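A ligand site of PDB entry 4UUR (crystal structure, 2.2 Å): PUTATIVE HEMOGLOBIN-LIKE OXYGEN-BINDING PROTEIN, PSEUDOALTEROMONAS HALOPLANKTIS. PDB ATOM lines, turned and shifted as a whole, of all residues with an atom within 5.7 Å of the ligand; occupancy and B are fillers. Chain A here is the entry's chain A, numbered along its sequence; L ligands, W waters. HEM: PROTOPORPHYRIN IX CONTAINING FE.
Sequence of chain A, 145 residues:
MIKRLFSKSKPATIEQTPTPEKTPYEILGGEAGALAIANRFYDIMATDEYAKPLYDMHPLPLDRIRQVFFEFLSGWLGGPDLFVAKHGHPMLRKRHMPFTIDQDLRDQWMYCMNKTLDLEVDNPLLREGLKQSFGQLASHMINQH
FE of the ligand is bound by NE2 of His 96, at 2.2 Å.
The guanidinium group of Arg 95 is in salt-bridge range of an oxygen (O2D) of the ligand (2.9 Å).
A ring nitrogen (ND1) of His 96 sits at hydrogen-bond distance from the backbone carbonyl oxygen of Leu 92 (2.7 Å).
A ring nitrogen (ND1) of His 96 is in hydrogen-bond range of the side-chain sulfur (SD) of Met 141 (3.5 Å).
The backbone carbonyl oxygen (O) of His 87 lies within hydrogen-bond range of the guanidinium group (NH2) of Arg 95 (2.8 Å).
The guanidinium group (NH2) of Arg 106 is in salt-bridge range of the side-chain carboxylate (OD1) of Asp 107, at 3.5 Å.
The backbone carbonyl oxygen of Leu 54 lies within hydrogen-bond range of a ring nitrogen (ND1) of His 58 (2.9 Å).
The backbone NH (N) of Leu 105 is in hydrogen-bond range of the side-chain carboxylate (OD1) of Asp 102 (2.9 Å).
The indole nitrogen of Trp 109 lies close to a nitrogen (NB) of the ligand (3.4 Å).
Residues that only touch the ligand: Leu 54 (3.4 Å), Met 57 (3.9 Å), His 58 (3.9 Å), Pro 59 (3.4 Å), Ile 65 (3.6 Å), Val 68 (3.7 Å), Phe 69 (3.996 Å), Phe 72 (3.6 Å), Leu 92 (3.4 Å), Phe 99 (3.5 Å), Ile 101 (3.3 Å), Leu 105 (3.7 Å), Arg 106 (3.2 Å), Phe 134 (3.9 Å), Leu 137 (3.6 Å), Ala 138 (3.7 Å) and Met 141 (3.8 Å).
Hydrophobic or aromatic side chains that line the ligand: Leu 54, Met 57, His 58, Pro 59, Ile 65, Val 68, Phe 69, Phe 72, Leu 92, His 96, Phe 99, Ile 101, Trp 109, Phe 134, Leu 137 and Met 141.
Within 4 Å of the ligand: Leu 54, Met 57, His 58, Pro 59, Ile 65, Val 68, Phe 69, Phe 72, Leu 92, Arg 95, His 96, Phe 99, Ile 101, Leu 105, Arg 106, Trp 109, Phe 134, Leu 137, Ala 138 and Met 141.
The nearest printed residue that does not touch the ligand is Phe 83 (4.005 Å).
Water W1 bridges the backbone carbonyl oxygen (O) of Pro 59 (2.9 Å) and an oxygen (O1A) of the ligand (3.0 Å).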
ATOM      1  N   TYR A  42     -36.597  21.197  -1.194  1.00  0.00           N
ATOM      2  CA  TYR A  42     -37.144  22.272  -2.022  1.00  0.00           C
ATOM      3  C   TYR A  42     -38.663  22.219  -2.041  1.00  0.00           C
ATOM      4  O   TYR A  42     -39.326  23.249  -2.144  1.00  0.00           O
ATOM      5  CB  TYR A  42     -36.546  22.160  -3.440  1.00  0.00           C
ATOM      6  CG  TYR A  42     -35.068  22.594  -3.458  1.00  0.00           C
ATOM      7  CD1 TYR A  42     -34.720  23.899  -3.131  1.00  0.00           C
ATOM      8  CD2 TYR A  42     -34.061  21.719  -3.744  1.00  0.00           C
ATOM      9  CE1 TYR A  42     -33.392  24.311  -3.061  1.00  0.00           C
ATOM     10  CE2 TYR A  42     -32.729  22.113  -3.730  1.00  0.00           C
ATOM     11  CZ  TYR A  42     -32.386  23.422  -3.382  1.00  0.00           C
ATOM     12  OH  TYR A  42     -31.066  23.861  -3.319  1.00  0.00           O
ATOM     13  N   LEU A  54     -36.292  32.831   1.936  1.00  0.00           N
ATOM     14  CA  LEU A  54     -35.283  31.968   1.344  1.00  0.00           C
ATOM     15  C   LEU A  54     -35.697  31.486  -0.046  1.00  0.00           C
ATOM     16  O   LEU A  54     -34.885  31.446  -0.969  1.00  0.00           O
ATOM     17  CB  LEU A  54     -35.001  30.824   2.291  1.00  0.00           C
ATOM     18  CG  LEU A  54     -34.096  29.692   1.799  1.00  0.00           C
ATOM     19  CD1 LEU A  54     -32.746  30.207   1.369  1.00  0.00           C
ATOM     20  CD2 LEU A  54     -33.961  28.634   2.902  1.00  0.00           C
ATOM     21  N   MET A  57     -35.166  33.952  -3.015  1.00  0.00           N
ATOM     22  CA  MET A  57     -33.847  34.117  -3.560  1.00  0.00           C
ATOM     23  C   MET A  57     -33.607  33.152  -4.743  1.00  0.00           C
ATOM     24  O   MET A  57     -32.610  33.260  -5.478  1.00  0.00           O
ATOM     25  CB  MET A  57     -32.815  33.832  -2.484  1.00  0.00           C
ATOM     26  CG  MET A  57     -32.928  34.670  -1.234  1.00  0.00           C
ATOM     27  SD  MET A  57     -31.670  34.107  -0.086  1.00  0.00           S
ATOM     28  CE  MET A  57     -30.207  34.889  -0.745  1.00  0.00           C
ATOM     29  N   HIS A  58     -34.530  32.227  -4.945  1.00  0.00           N
ATOM     30  CA  HIS A  58     -34.339  31.240  -6.004  1.00  0.00           C
ATOM     31  C   HIS A  58     -35.152  31.617  -7.246  1.00  0.00           C
ATOM     32  O   HIS A  58     -36.357  31.535  -7.228  1.00  0.00           O
ATOM     33  CB  HIS A  58     -34.753  29.856  -5.522  1.00  0.00           C
ATOM     34  CG  HIS A  58     -33.872  29.300  -4.449  1.00  0.00           C
ATOM     35  ND1 HIS A  58     -33.939  29.709  -3.132  1.00  0.00           N
ATOM     36  CD2 HIS A  58     -32.923  28.335  -4.502  1.00  0.00           C
ATOM     37  CE1 HIS A  58     -33.055  29.021  -2.423  1.00  0.00           C
ATOM     38  NE2 HIS A  58     -32.445  28.167  -3.230  1.00  0.00           N
ATOM     39  N   PRO A  59     -34.492  31.990  -8.350  1.00  0.00           N
ATOM     40  CA  PRO A  59     -35.218  32.223  -9.600  1.00  0.00           C
ATOM     41  C   PRO A  59     -35.811  30.921 -10.116  1.00  0.00           C
ATOM     42  O   PRO A  59     -35.161  29.871 -10.069  1.00  0.00           O
ATOM     43  CB  PRO A  59     -34.118  32.732 -10.560  1.00  0.00           C
ATOM     44  CG  PRO A  59     -32.896  32.887  -9.730  1.00  0.00           C
ATOM     45  CD  PRO A  59     -33.040  31.949  -8.578  1.00  0.00           C
ATOM     46  N   ARG A  64     -33.002  22.986 -12.134  1.00  0.00           N
ATOM     47  CA  ARG A  64     -31.539  22.862 -12.133  1.00  0.00           C
ATOM     48  C   ARG A  64     -30.966  22.789 -10.715  1.00  0.00           C
ATOM     49  O   ARG A  64     -30.058  21.971 -10.493  1.00  0.00           O
ATOM     50  CB  ARG A  64     -30.903  24.011 -12.962  1.00  0.00           C
ATOM     51  CG  ARG A  64     -29.591  24.624 -12.464  1.00  0.00           C
ATOM     52  CD  ARG A  64     -28.339  23.966 -13.071  1.00  0.00           C
ATOM     53  NE  ARG A  64     -27.163  24.841 -13.303  1.00  0.00           N
ATOM     54  CZ  ARG A  64     -26.774  25.905 -12.575  1.00  0.00           C
ATOM     55  NH1 ARG A  64     -27.422  26.324 -11.504  1.00  0.00           N
ATOM     56  NH2 ARG A  64     -25.687  26.555 -12.950  1.00  0.00           N
ATOM     57  N   ILE A  65     -31.452  23.648  -9.788  1.00  0.00           N
ATOM     58  CA  ILE A  65     -30.911  23.635  -8.427  1.00  0.00           C
ATOM     59  C   ILE A  65     -31.310  22.354  -7.673  1.00  0.00           C
ATOM     60  O   ILE A  65     -30.549  21.863  -6.835  1.00  0.00           O
ATOM     61  CB  ILE A  65     -31.325  24.908  -7.631  1.00  0.00           C
ATOM     62  CG1 ILE A  65     -30.619  24.970  -6.304  1.00  0.00           C
ATOM     63  CG2 ILE A  65     -32.822  24.921  -7.343  1.00  0.00           C
ATOM     64  CD1 ILE A  65     -29.123  24.981  -6.416  1.00  0.00           C
ATOM     65  N   VAL A  68     -28.651  20.037  -9.120  1.00  0.00           N
ATOM     66  CA  VAL A  68     -27.324  20.411  -8.609  1.00  0.00           C
ATOM     67  C   VAL A  68     -27.171  20.052  -7.147  1.00  0.00           C
ATOM     68  O   VAL A  68     -26.183  19.454  -6.760  1.00  0.00           O
ATOM     69  CB  VAL A  68     -27.027  21.894  -8.809  1.00  0.00           C
ATOM     70  CG1 VAL A  68     -25.770  22.326  -8.054  1.00  0.00           C
ATOM     71  CG2 VAL A  68     -26.820  22.169 -10.292  1.00  0.00           C
ATOM     72  N   PHE A  69     -28.150  20.415  -6.315  1.00  0.00           N
ATOM     73  CA  PHE A  69     -28.072  20.098  -4.878  1.00  0.00           C
ATOM     74  C   PHE A  69     -27.973  18.591  -4.688  1.00  0.00           C
ATOM     75  O   PHE A  69     -27.233  18.148  -3.836  1.00  0.00           O
ATOM     76  CB  PHE A  69     -29.302  20.615  -4.126  1.00  0.00           C
ATOM     77  CG  PHE A  69     -29.203  20.510  -2.633  1.00  0.00           C
ATOM     78  CD1 PHE A  69     -28.141  21.062  -1.954  1.00  0.00           C
ATOM     79  CD2 PHE A  69     -30.192  19.943  -1.913  1.00  0.00           C
ATOM     80  CE1 PHE A  69     -28.039  20.971  -0.575  1.00  0.00           C
ATOM     81  CE2 PHE A  69     -30.166  19.908  -0.538  1.00  0.00           C
ATOM     82  CZ  PHE A  69     -29.076  20.408   0.134  1.00  0.00           C
ATOM     83  N   PHE A  72     -24.614  17.474  -5.361  1.00  0.00           N
ATOM     84  CA  PHE A  72     -23.749  17.791  -4.208  1.00  0.00           C
ATOM     85  C   PHE A  72     -23.880  16.784  -3.104  1.00  0.00           C
ATOM     86  O   PHE A  72     -22.868  16.298  -2.581  1.00  0.00           O
ATOM     87  CB  PHE A  72     -23.998  19.182  -3.661  1.00  0.00           C
ATOM     88  CG  PHE A  72     -23.355  19.431  -2.343  1.00  0.00           C
ATOM     89  CD1 PHE A  72     -21.998  19.735  -2.249  1.00  0.00           C
ATOM     90  CD2 PHE A  72     -24.117  19.367  -1.164  1.00  0.00           C
ATOM     91  CE1 PHE A  72     -21.417  19.981  -1.005  1.00  0.00           C
ATOM     92  CE2 PHE A  72     -23.561  19.615   0.061  1.00  0.00           C
ATOM     93  CZ  PHE A  72     -22.193  19.924   0.147  1.00  0.00           C
ATOM     94  N   TRP A  76     -21.178  14.570  -0.878  1.00  0.00           N
ATOM     95  CA  TRP A  76     -21.074  14.956   0.542  1.00  0.00           C
ATOM     96  C   TRP A  76     -21.470  13.815   1.497  1.00  0.00           C
ATOM     97  O   TRP A  76     -21.072  13.826   2.669  1.00  0.00           O
ATOM     98  CB  TRP A  76     -21.964  16.156   0.803  1.00  0.00           C
ATOM     99  CG  TRP A  76     -21.762  16.777   2.082  1.00  0.00           C
ATOM    100  CD1 TRP A  76     -20.728  17.556   2.444  1.00  0.00           C
ATOM    101  CD2 TRP A  76     -22.685  16.779   3.199  1.00  0.00           C
ATOM    102  NE1 TRP A  76     -20.920  18.035   3.725  1.00  0.00           N
ATOM    103  CE2 TRP A  76     -22.107  17.556   4.207  1.00  0.00           C
ATOM    104  CE3 TRP A  76     -23.945  16.197   3.420  1.00  0.00           C
ATOM    105  CZ2 TRP A  76     -22.739  17.780   5.446  1.00  0.00           C
ATOM    106  CZ3 TRP A  76     -24.559  16.397   4.630  1.00  0.00           C
ATOM    107  CH2 TRP A  76     -23.965  17.187   5.630  1.00  0.00           C
ATOM    108  N   PHE A  83     -21.010  16.305  -8.040  1.00  0.00           N
ATOM    109  CA  PHE A  83     -20.805  17.753  -8.021  1.00  0.00           C
ATOM    110  C   PHE A  83     -19.394  18.049  -8.428  1.00  0.00           C
ATOM    111  O   PHE A  83     -19.180  18.651  -9.475  1.00  0.00           O
ATOM    112  CB  PHE A  83     -21.076  18.356  -6.633  1.00  0.00           C
ATOM    113  CG  PHE A  83     -21.055  19.867  -6.597  1.00  0.00           C
ATOM    114  CD1 PHE A  83     -19.882  20.564  -6.412  1.00  0.00           C
ATOM    115  CD2 PHE A  83     -22.248  20.589  -6.755  1.00  0.00           C
ATOM    116  CE1 PHE A  83     -19.876  21.954  -6.392  1.00  0.00           C
ATOM    117  CE2 PHE A  83     -22.248  21.983  -6.728  1.00  0.00           C
ATOM    118  CZ  PHE A  83     -21.071  22.655  -6.528  1.00  0.00           C
ATOM    119  N   HIS A  87     -18.866  20.297 -11.532  1.00  0.00           N
ATOM    120  CA  HIS A  87     -18.789  21.727 -11.192  1.00  0.00           C
ATOM    121  C   HIS A  87     -17.511  22.110 -10.451  1.00  0.00           C
ATOM    122  O   HIS A  87     -17.343  23.296 -10.173  1.00  0.00           O
ATOM    123  CB  HIS A  87     -20.023  22.159 -10.345  1.00  0.00           C
ATOM    124  CG  HIS A  87     -21.352  21.746 -10.933  1.00  0.00           C
ATOM    125  ND1 HIS A  87     -21.991  22.469 -11.921  1.00  0.00           N
ATOM    126  CD2 HIS A  87     -22.151  20.675 -10.691  1.00  0.00           C
ATOM    127  CE1 HIS A  87     -23.107  21.868 -12.262  1.00  0.00           C
ATOM    128  NE2 HIS A  87     -23.232  20.774 -11.531  1.00  0.00           N
ATOM    129  N   LEU A  92     -18.271  26.051  -0.756  1.00  0.00           N
ATOM    130  CA  LEU A  92     -19.628  26.533  -0.548  1.00  0.00           C
ATOM    131  C   LEU A  92     -19.678  27.957  -0.030  1.00  0.00           C
ATOM    132  O   LEU A  92     -20.518  28.729  -0.502  1.00  0.00           O
ATOM    133  CB  LEU A  92     -20.417  25.646   0.410  1.00  0.00           C
ATOM    134  CG  LEU A  92     -20.715  24.230  -0.093  1.00  0.00           C
ATOM    135  CD1 LEU A  92     -21.760  23.607   0.846  1.00  0.00           C
ATOM    136  CD2 LEU A  92     -21.189  24.209  -1.550  1.00  0.00           C
ATOM    137  N   ARG A  95     -18.981  30.205  -3.046  1.00  0.00           N
ATOM    138  CA  ARG A  95     -20.126  30.046  -3.951  1.00  0.00           C
ATOM    139  C   ARG A  95     -21.401  30.763  -3.529  1.00  0.00           C
ATOM    140  O   ARG A  95     -22.153  31.143  -4.385  1.00  0.00           O
ATOM    141  CB  ARG A  95     -20.443  28.572  -4.111  1.00  0.00           C
ATOM    142  CG  ARG A  95     -19.783  27.975  -5.312  1.00  0.00           C
ATOM    143  CD  ARG A  95     -20.383  26.612  -5.585  1.00  0.00           C
ATOM    144  NE  ARG A  95     -19.878  26.034  -6.819  1.00  0.00           N
ATOM    145  CZ  ARG A  95     -18.672  25.483  -6.930  1.00  0.00           C
ATOM    146  NH1 ARG A  95     -17.855  25.449  -5.890  1.00  0.00           N
ATOM    147  NH2 ARG A  95     -18.298  24.953  -8.072  1.00  0.00           N
ATOM    148  N   HIS A  96     -21.629  30.941  -2.215  1.00  0.00           N
ATOM    149  CA  HIS A  96     -22.720  31.792  -1.668  1.00  0.00           C
ATOM    150  C   HIS A  96     -22.413  33.249  -1.493  1.00  0.00           C
ATOM    151  O   HIS A  96     -23.312  34.022  -1.111  1.00  0.00           O
ATOM    152  CB  HIS A  96     -23.199  31.261  -0.315  1.00  0.00           C
ATOM    153  CG  HIS A  96     -23.881  29.945  -0.442  1.00  0.00           C
ATOM    154  ND1 HIS A  96     -23.201  28.794  -0.755  1.00  0.00           N
ATOM    155  CD2 HIS A  96     -25.187  29.620  -0.417  1.00  0.00           C
ATOM    156  CE1 HIS A  96     -24.061  27.803  -0.887  1.00  0.00           C
ATOM    157  NE2 HIS A  96     -25.272  28.282  -0.675  1.00  0.00           N
ATOM    158  N   PHE A  99     -24.607  36.215  -2.655  1.00  0.00           N
ATOM    159  CA  PHE A  99     -25.854  36.508  -1.924  1.00  0.00           C
ATOM    160  C   PHE A  99     -25.558  37.139  -0.552  1.00  0.00           C
ATOM    161  O   PHE A  99     -24.463  37.014   0.025  1.00  0.00           O
ATOM    162  CB  PHE A  99     -26.723  35.240  -1.770  1.00  0.00           C
ATOM    163  CG  PHE A  99     -26.737  34.350  -2.996  1.00  0.00           C
ATOM    164  CD1 PHE A  99     -27.455  34.714  -4.131  1.00  0.00           C
ATOM    165  CD2 PHE A  99     -26.025  33.177  -3.027  1.00  0.00           C
ATOM    166  CE1 PHE A  99     -27.475  33.904  -5.267  1.00  0.00           C
ATOM    167  CE2 PHE A  99     -25.999  32.375  -4.159  1.00  0.00           C
ATOM    168  CZ  PHE A  99     -26.733  32.738  -5.278  1.00  0.00           C
ATOM    169  N   ILE A 101     -26.524  36.620   3.051  1.00  0.00           N
ATOM    170  CA  ILE A 101     -27.066  35.572   3.942  1.00  0.00           C
ATOM    171  C   ILE A 101     -26.858  35.935   5.412  1.00  0.00           C
ATOM    172  O   ILE A 101     -25.724  35.898   5.893  1.00  0.00           O
ATOM    173  CB  ILE A 101     -26.330  34.263   3.658  1.00  0.00           C
ATOM    174  CG1 ILE A 101     -26.491  33.895   2.199  1.00  0.00           C
ATOM    175  CG2 ILE A 101     -26.830  33.157   4.584  1.00  0.00           C
ATOM    176  CD1 ILE A 101     -25.648  32.724   1.791  1.00  0.00           C
ATOM    177  N   ASP A 102     -27.943  36.282   6.103  1.00  0.00           N
ATOM    178  CA  ASP A 102     -27.918  36.531   7.561  1.00  0.00           C
ATOM    179  C   ASP A 102     -28.409  35.309   8.390  1.00  0.00           C
ATOM    180  O   ASP A 102     -28.777  34.267   7.831  1.00  0.00           O
ATOM    181  CB  ASP A 102     -28.770  37.774   7.925  1.00  0.00           C
ATOM    182  CG  ASP A 102     -30.195  37.635   7.462  1.00  0.00           C
ATOM    183  OD1 ASP A 102     -30.590  36.486   7.142  1.00  0.00           O
ATOM    184  OD2 ASP A 102     -30.920  38.644   7.364  1.00  0.00           O
ATOM    185  N   LEU A 105     -31.857  33.873   7.470  1.00  0.00           N
ATOM    186  CA  LEU A 105     -31.908  32.998   6.317  1.00  0.00           C
ATOM    187  C   LEU A 105     -31.255  31.660   6.586  1.00  0.00           C
ATOM    188  O   LEU A 105     -31.721  30.656   6.080  1.00  0.00           O
ATOM    189  CB  LEU A 105     -31.288  33.663   5.071  1.00  0.00           C
ATOM    190  CG  LEU A 105     -32.061  34.827   4.461  1.00  0.00           C
ATOM    191  CD1 LEU A 105     -31.147  35.606   3.491  1.00  0.00           C
ATOM    192  CD2 LEU A 105     -33.327  34.347   3.779  1.00  0.00           C
ATOM    193  N   ARG A 106     -30.184  31.645   7.360  1.00  0.00           N
ATOM    194  CA  ARG A 106     -29.618  30.407   7.837  1.00  0.00           C
ATOM    195  C   ARG A 106     -30.649  29.542   8.598  1.00  0.00           C
ATOM    196  O   ARG A 106     -30.723  28.330   8.393  1.00  0.00           O
ATOM    197  CB  ARG A 106     -28.443  30.642   8.752  1.00  0.00           C
ATOM    198  CG  ARG A 106     -27.569  29.397   8.869  1.00  0.00           C
ATOM    199  CD  ARG A 106     -27.131  29.078  10.311  1.00  0.00           C
ATOM    200  NE  ARG A 106     -28.193  28.466  11.095  1.00  0.00           N
ATOM    201  CZ  ARG A 106     -28.119  27.335  11.806  1.00  0.00           C
ATOM    202  NH1 ARG A 106     -27.005  26.610  11.919  1.00  0.00           N
ATOM    203  NH2 ARG A 106     -29.198  26.930  12.428  1.00  0.00           N
ATOM    204  N   ASP A 107     -31.439  30.169   9.452  1.00  0.00           N
ATOM    205  CA  ASP A 107     -32.415  29.437  10.255  1.00  0.00           C
ATOM    206  C   ASP A 107     -33.552  28.883   9.411  1.00  0.00           C
ATOM    207  O   ASP A 107     -34.011  27.788   9.667  1.00  0.00           O
ATOM    208  CB  ASP A 107     -32.996  30.330  11.363  1.00  0.00           C
ATOM    209  CG  ASP A 107     -31.976  30.679  12.442  1.00  0.00           C
ATOM    210  OD1 ASP A 107     -31.014  29.937  12.693  1.00  0.00           O
ATOM    211  OD2 ASP A 107     -32.157  31.733  13.051  1.00  0.00           O
ATOM    212  N   TRP A 109     -33.184  28.029   6.237  1.00  0.00           N
ATOM    213  CA  TRP A 109     -32.552  26.913   5.529  1.00  0.00           C
ATOM    214  C   TRP A 109     -32.509  25.699   6.437  1.00  0.00           C
ATOM    215  O   TRP A 109     -32.847  24.588   5.991  1.00  0.00           O
ATOM    216  CB  TRP A 109     -31.119  27.257   5.156  1.00  0.00           C
ATOM    217  CG  TRP A 109     -30.566  26.472   4.038  1.00  0.00           C
ATOM    218  CD1 TRP A 109     -30.479  26.864   2.730  1.00  0.00           C
ATOM    219  CD2 TRP A 109     -30.039  25.158   4.088  1.00  0.00           C
ATOM    220  NE1 TRP A 109     -29.890  25.886   1.971  1.00  0.00           N
ATOM    221  CE2 TRP A 109     -29.600  24.822   2.787  1.00  0.00           C
ATOM    222  CE3 TRP A 109     -29.839  24.230   5.104  1.00  0.00           C
ATOM    223  CZ2 TRP A 109     -29.017  23.589   2.483  1.00  0.00           C
ATOM    224  CZ3 TRP A 109     -29.223  23.000   4.783  1.00  0.00           C
ATOM    225  CH2 TRP A 109     -28.848  22.704   3.521  1.00  0.00           C
ATOM    226  N   PHE A 134     -25.011  19.642   8.762  1.00  0.00           N
ATOM    227  CA  PHE A 134     -25.698  20.711   8.007  1.00  0.00           C
ATOM    228  C   PHE A 134     -25.743  22.010   8.799  1.00  0.00           C
ATOM    229  O   PHE A 134     -25.498  23.070   8.246  1.00  0.00           O
ATOM    230  CB  PHE A 134     -27.169  20.348   7.625  1.00  0.00           C
ATOM    231  CG  PHE A 134     -27.286  19.406   6.443  1.00  0.00           C
ATOM    232  CD1 PHE A 134     -26.926  19.826   5.166  1.00  0.00           C
ATOM    233  CD2 PHE A 134     -27.814  18.147   6.596  1.00  0.00           C
ATOM    234  CE1 PHE A 134     -27.043  18.972   4.088  1.00  0.00           C
ATOM    235  CE2 PHE A 134     -27.919  17.286   5.516  1.00  0.00           C
ATOM    236  CZ  PHE A 134     -27.551  17.691   4.253  1.00  0.00           C
ATOM    237  N   LEU A 137     -22.314  23.764   8.449  1.00  0.00           N
ATOM    238  CA  LEU A 137     -22.231  24.293   7.080  1.00  0.00           C
ATOM    239  C   LEU A 137     -23.088  25.533   6.856  1.00  0.00           C
ATOM    240  O   LEU A 137     -22.584  26.540   6.380  1.00  0.00           O
ATOM    241  CB  LEU A 137     -22.604  23.222   6.067  1.00  0.00           C
ATOM    242  CG  LEU A 137     -21.383  22.538   5.492  1.00  0.00           C
ATOM    243  CD1 LEU A 137     -21.819  21.534   4.410  1.00  0.00           C
ATOM    244  CD2 LEU A 137     -20.425  23.585   4.921  1.00  0.00           C
ATOM    245  N   ALA A 138     -24.351  25.476   7.266  1.00  0.00           N
ATOM    246  CA  ALA A 138     -25.268  26.620   7.155  1.00  0.00           C
ATOM    247  C   ALA A 138     -24.746  27.827   7.870  1.00  0.00           C
ATOM    248  O   ALA A 138     -24.777  28.908   7.313  1.00  0.00           O
ATOM    249  CB  ALA A 138     -26.644  26.303   7.708  1.00  0.00           C
ATOM    250  N   MET A 141     -21.956  29.663   6.006  1.00  0.00           N
ATOM    251  CA  MET A 141     -22.330  30.473   4.835  1.00  0.00           C
ATOM    252  C   MET A 141     -22.707  31.881   5.220  1.00  0.00           C
ATOM    253  O   MET A 141     -22.758  32.756   4.359  1.00  0.00           O
ATOM    254  CB  MET A 141     -23.557  29.910   4.118  1.00  0.00           C
ATOM    255  CG  MET A 141     -23.491  28.482   3.655  1.00  0.00           C
ATOM    256  SD  MET A 141     -22.135  28.238   2.532  1.00  0.00           S
ATOM    257  CE  MET A 141     -20.912  27.469   3.597  1.00  0.00           C
ATOM    258  N   ILE A 142     -23.023  32.096   6.488  1.00  0.00           N
ATOM    259  CA  ILE A 142     -23.559  33.381   6.937  1.00  0.00           C
ATOM    260  C   ILE A 142     -22.485  34.386   6.558  1.00  0.00           C
ATOM    261  O   ILE A 142     -21.320  34.128   6.810  1.00  0.00           O
ATOM    262  CB  ILE A 142     -23.801  33.396   8.448  1.00  0.00           C
ATOM    263  CG1 ILE A 142     -24.996  32.494   8.788  1.00  0.00           C
ATOM    264  CG2 ILE A 142     -24.025  34.829   8.977  1.00  0.00           C
ATOM    265  CD1 ILE A 142     -25.744  32.823  10.074  1.00  0.00           C
HETATM  266  CHA HEM L   1     -26.884  27.437  -4.173  1.00  0.00           C
HETATM  267  CHB HEM L   1     -29.029  29.972  -0.617  1.00  0.00           C
HETATM  268  CHC HEM L   1     -26.829  27.064   2.592  1.00  0.00           C
HETATM  269  CHD HEM L   1     -25.608  24.118  -0.968  1.00  0.00           C
HETATM  270  C1A HEM L   1     -27.620  28.379  -3.495  1.00  0.00           C
HETATM  271  C2A HEM L   1     -28.358  29.407  -4.103  1.00  0.00           C
HETATM  272  C3A HEM L   1     -28.981  30.096  -3.099  1.00  0.00           C
HETATM  273  C4A HEM L   1     -28.622  29.520  -1.856  1.00  0.00           C
HETATM  274  CMA HEM L   1     -29.891  31.313  -3.269  1.00  0.00           C
HETATM  275  CAA HEM L   1     -28.468  29.728  -5.581  1.00  0.00           C
HETATM  276  CBA HEM L   1     -28.977  28.552  -6.411  1.00  0.00           C
HETATM  277  CGA HEM L   1     -29.793  28.921  -7.624  1.00  0.00           C
HETATM  278  O1A HEM L   1     -30.922  29.456  -7.596  1.00  0.00           O
HETATM  279  O2A HEM L   1     -29.314  28.610  -8.730  1.00  0.00           O
HETATM  280  C1B HEM L   1     -28.574  29.407   0.583  1.00  0.00           C
HETATM  281  C2B HEM L   1     -28.761  29.978   1.875  1.00  0.00           C
HETATM  282  C3B HEM L   1     -28.131  29.162   2.781  1.00  0.00           C
HETATM  283  C4B HEM L   1     -27.505  28.113   1.979  1.00  0.00           C
HETATM  284  CMB HEM L   1     -29.599  31.228   2.124  1.00  0.00           C
HETATM  285  CAB HEM L   1     -27.901  29.142   4.263  1.00  0.00           C
HETATM  286  CBB HEM L   1     -28.196  30.145   5.016  1.00  0.00           C
HETATM  287  C1C HEM L   1     -26.367  25.935   1.924  1.00  0.00           C
HETATM  288  C2C HEM L   1     -25.861  24.764   2.523  1.00  0.00           C
HETATM  289  C3C HEM L   1     -25.497  23.945   1.483  1.00  0.00           C
HETATM  290  C4C HEM L   1     -25.827  24.610   0.271  1.00  0.00           C
HETATM  291  CMC HEM L   1     -25.723  24.532   4.018  1.00  0.00           C
HETATM  292  CAC HEM L   1     -24.939  22.575   1.490  1.00  0.00           C
HETATM  293  CBC HEM L   1     -24.860  21.840   2.600  1.00  0.00           C
HETATM  294  C1D HEM L   1     -25.834  24.856  -2.097  1.00  0.00           C
HETATM  295  C2D HEM L   1     -25.404  24.363  -3.392  1.00  0.00           C
HETATM  296  C3D HEM L   1     -25.756  25.274  -4.270  1.00  0.00           C
HETATM  297  C4D HEM L   1     -26.392  26.337  -3.511  1.00  0.00           C
HETATM  298  CMD HEM L   1     -24.671  23.098  -3.741  1.00  0.00           C
HETATM  299  CAD HEM L   1     -25.473  25.259  -5.763  1.00  0.00           C
HETATM  300  CBD HEM L   1     -24.207  26.085  -5.942  1.00  0.00           C
HETATM  301  CGD HEM L   1     -23.669  26.123  -7.375  1.00  0.00           C
HETATM  302  O1D HEM L   1     -24.299  25.658  -8.340  1.00  0.00           O
HETATM  303  O2D HEM L   1     -22.563  26.629  -7.648  1.00  0.00           O
HETATM  304  NA  HEM L   1     -27.840  28.441  -2.114  1.00  0.00           N
HETATM  305  NB  HEM L   1     -27.835  28.322   0.718  1.00  0.00           N
HETATM  306  NC  HEM L   1     -26.364  25.794   0.595  1.00  0.00           N
HETATM  307  ND  HEM L   1     -26.467  26.008  -2.198  1.00  0.00           N
HETATM  308 FE   HEM L   1     -27.099  27.112  -0.816  1.00  0.00          FE
HETATM  309  O   HOH W   1     -33.401  28.168  -8.584  1.00  0.00           O
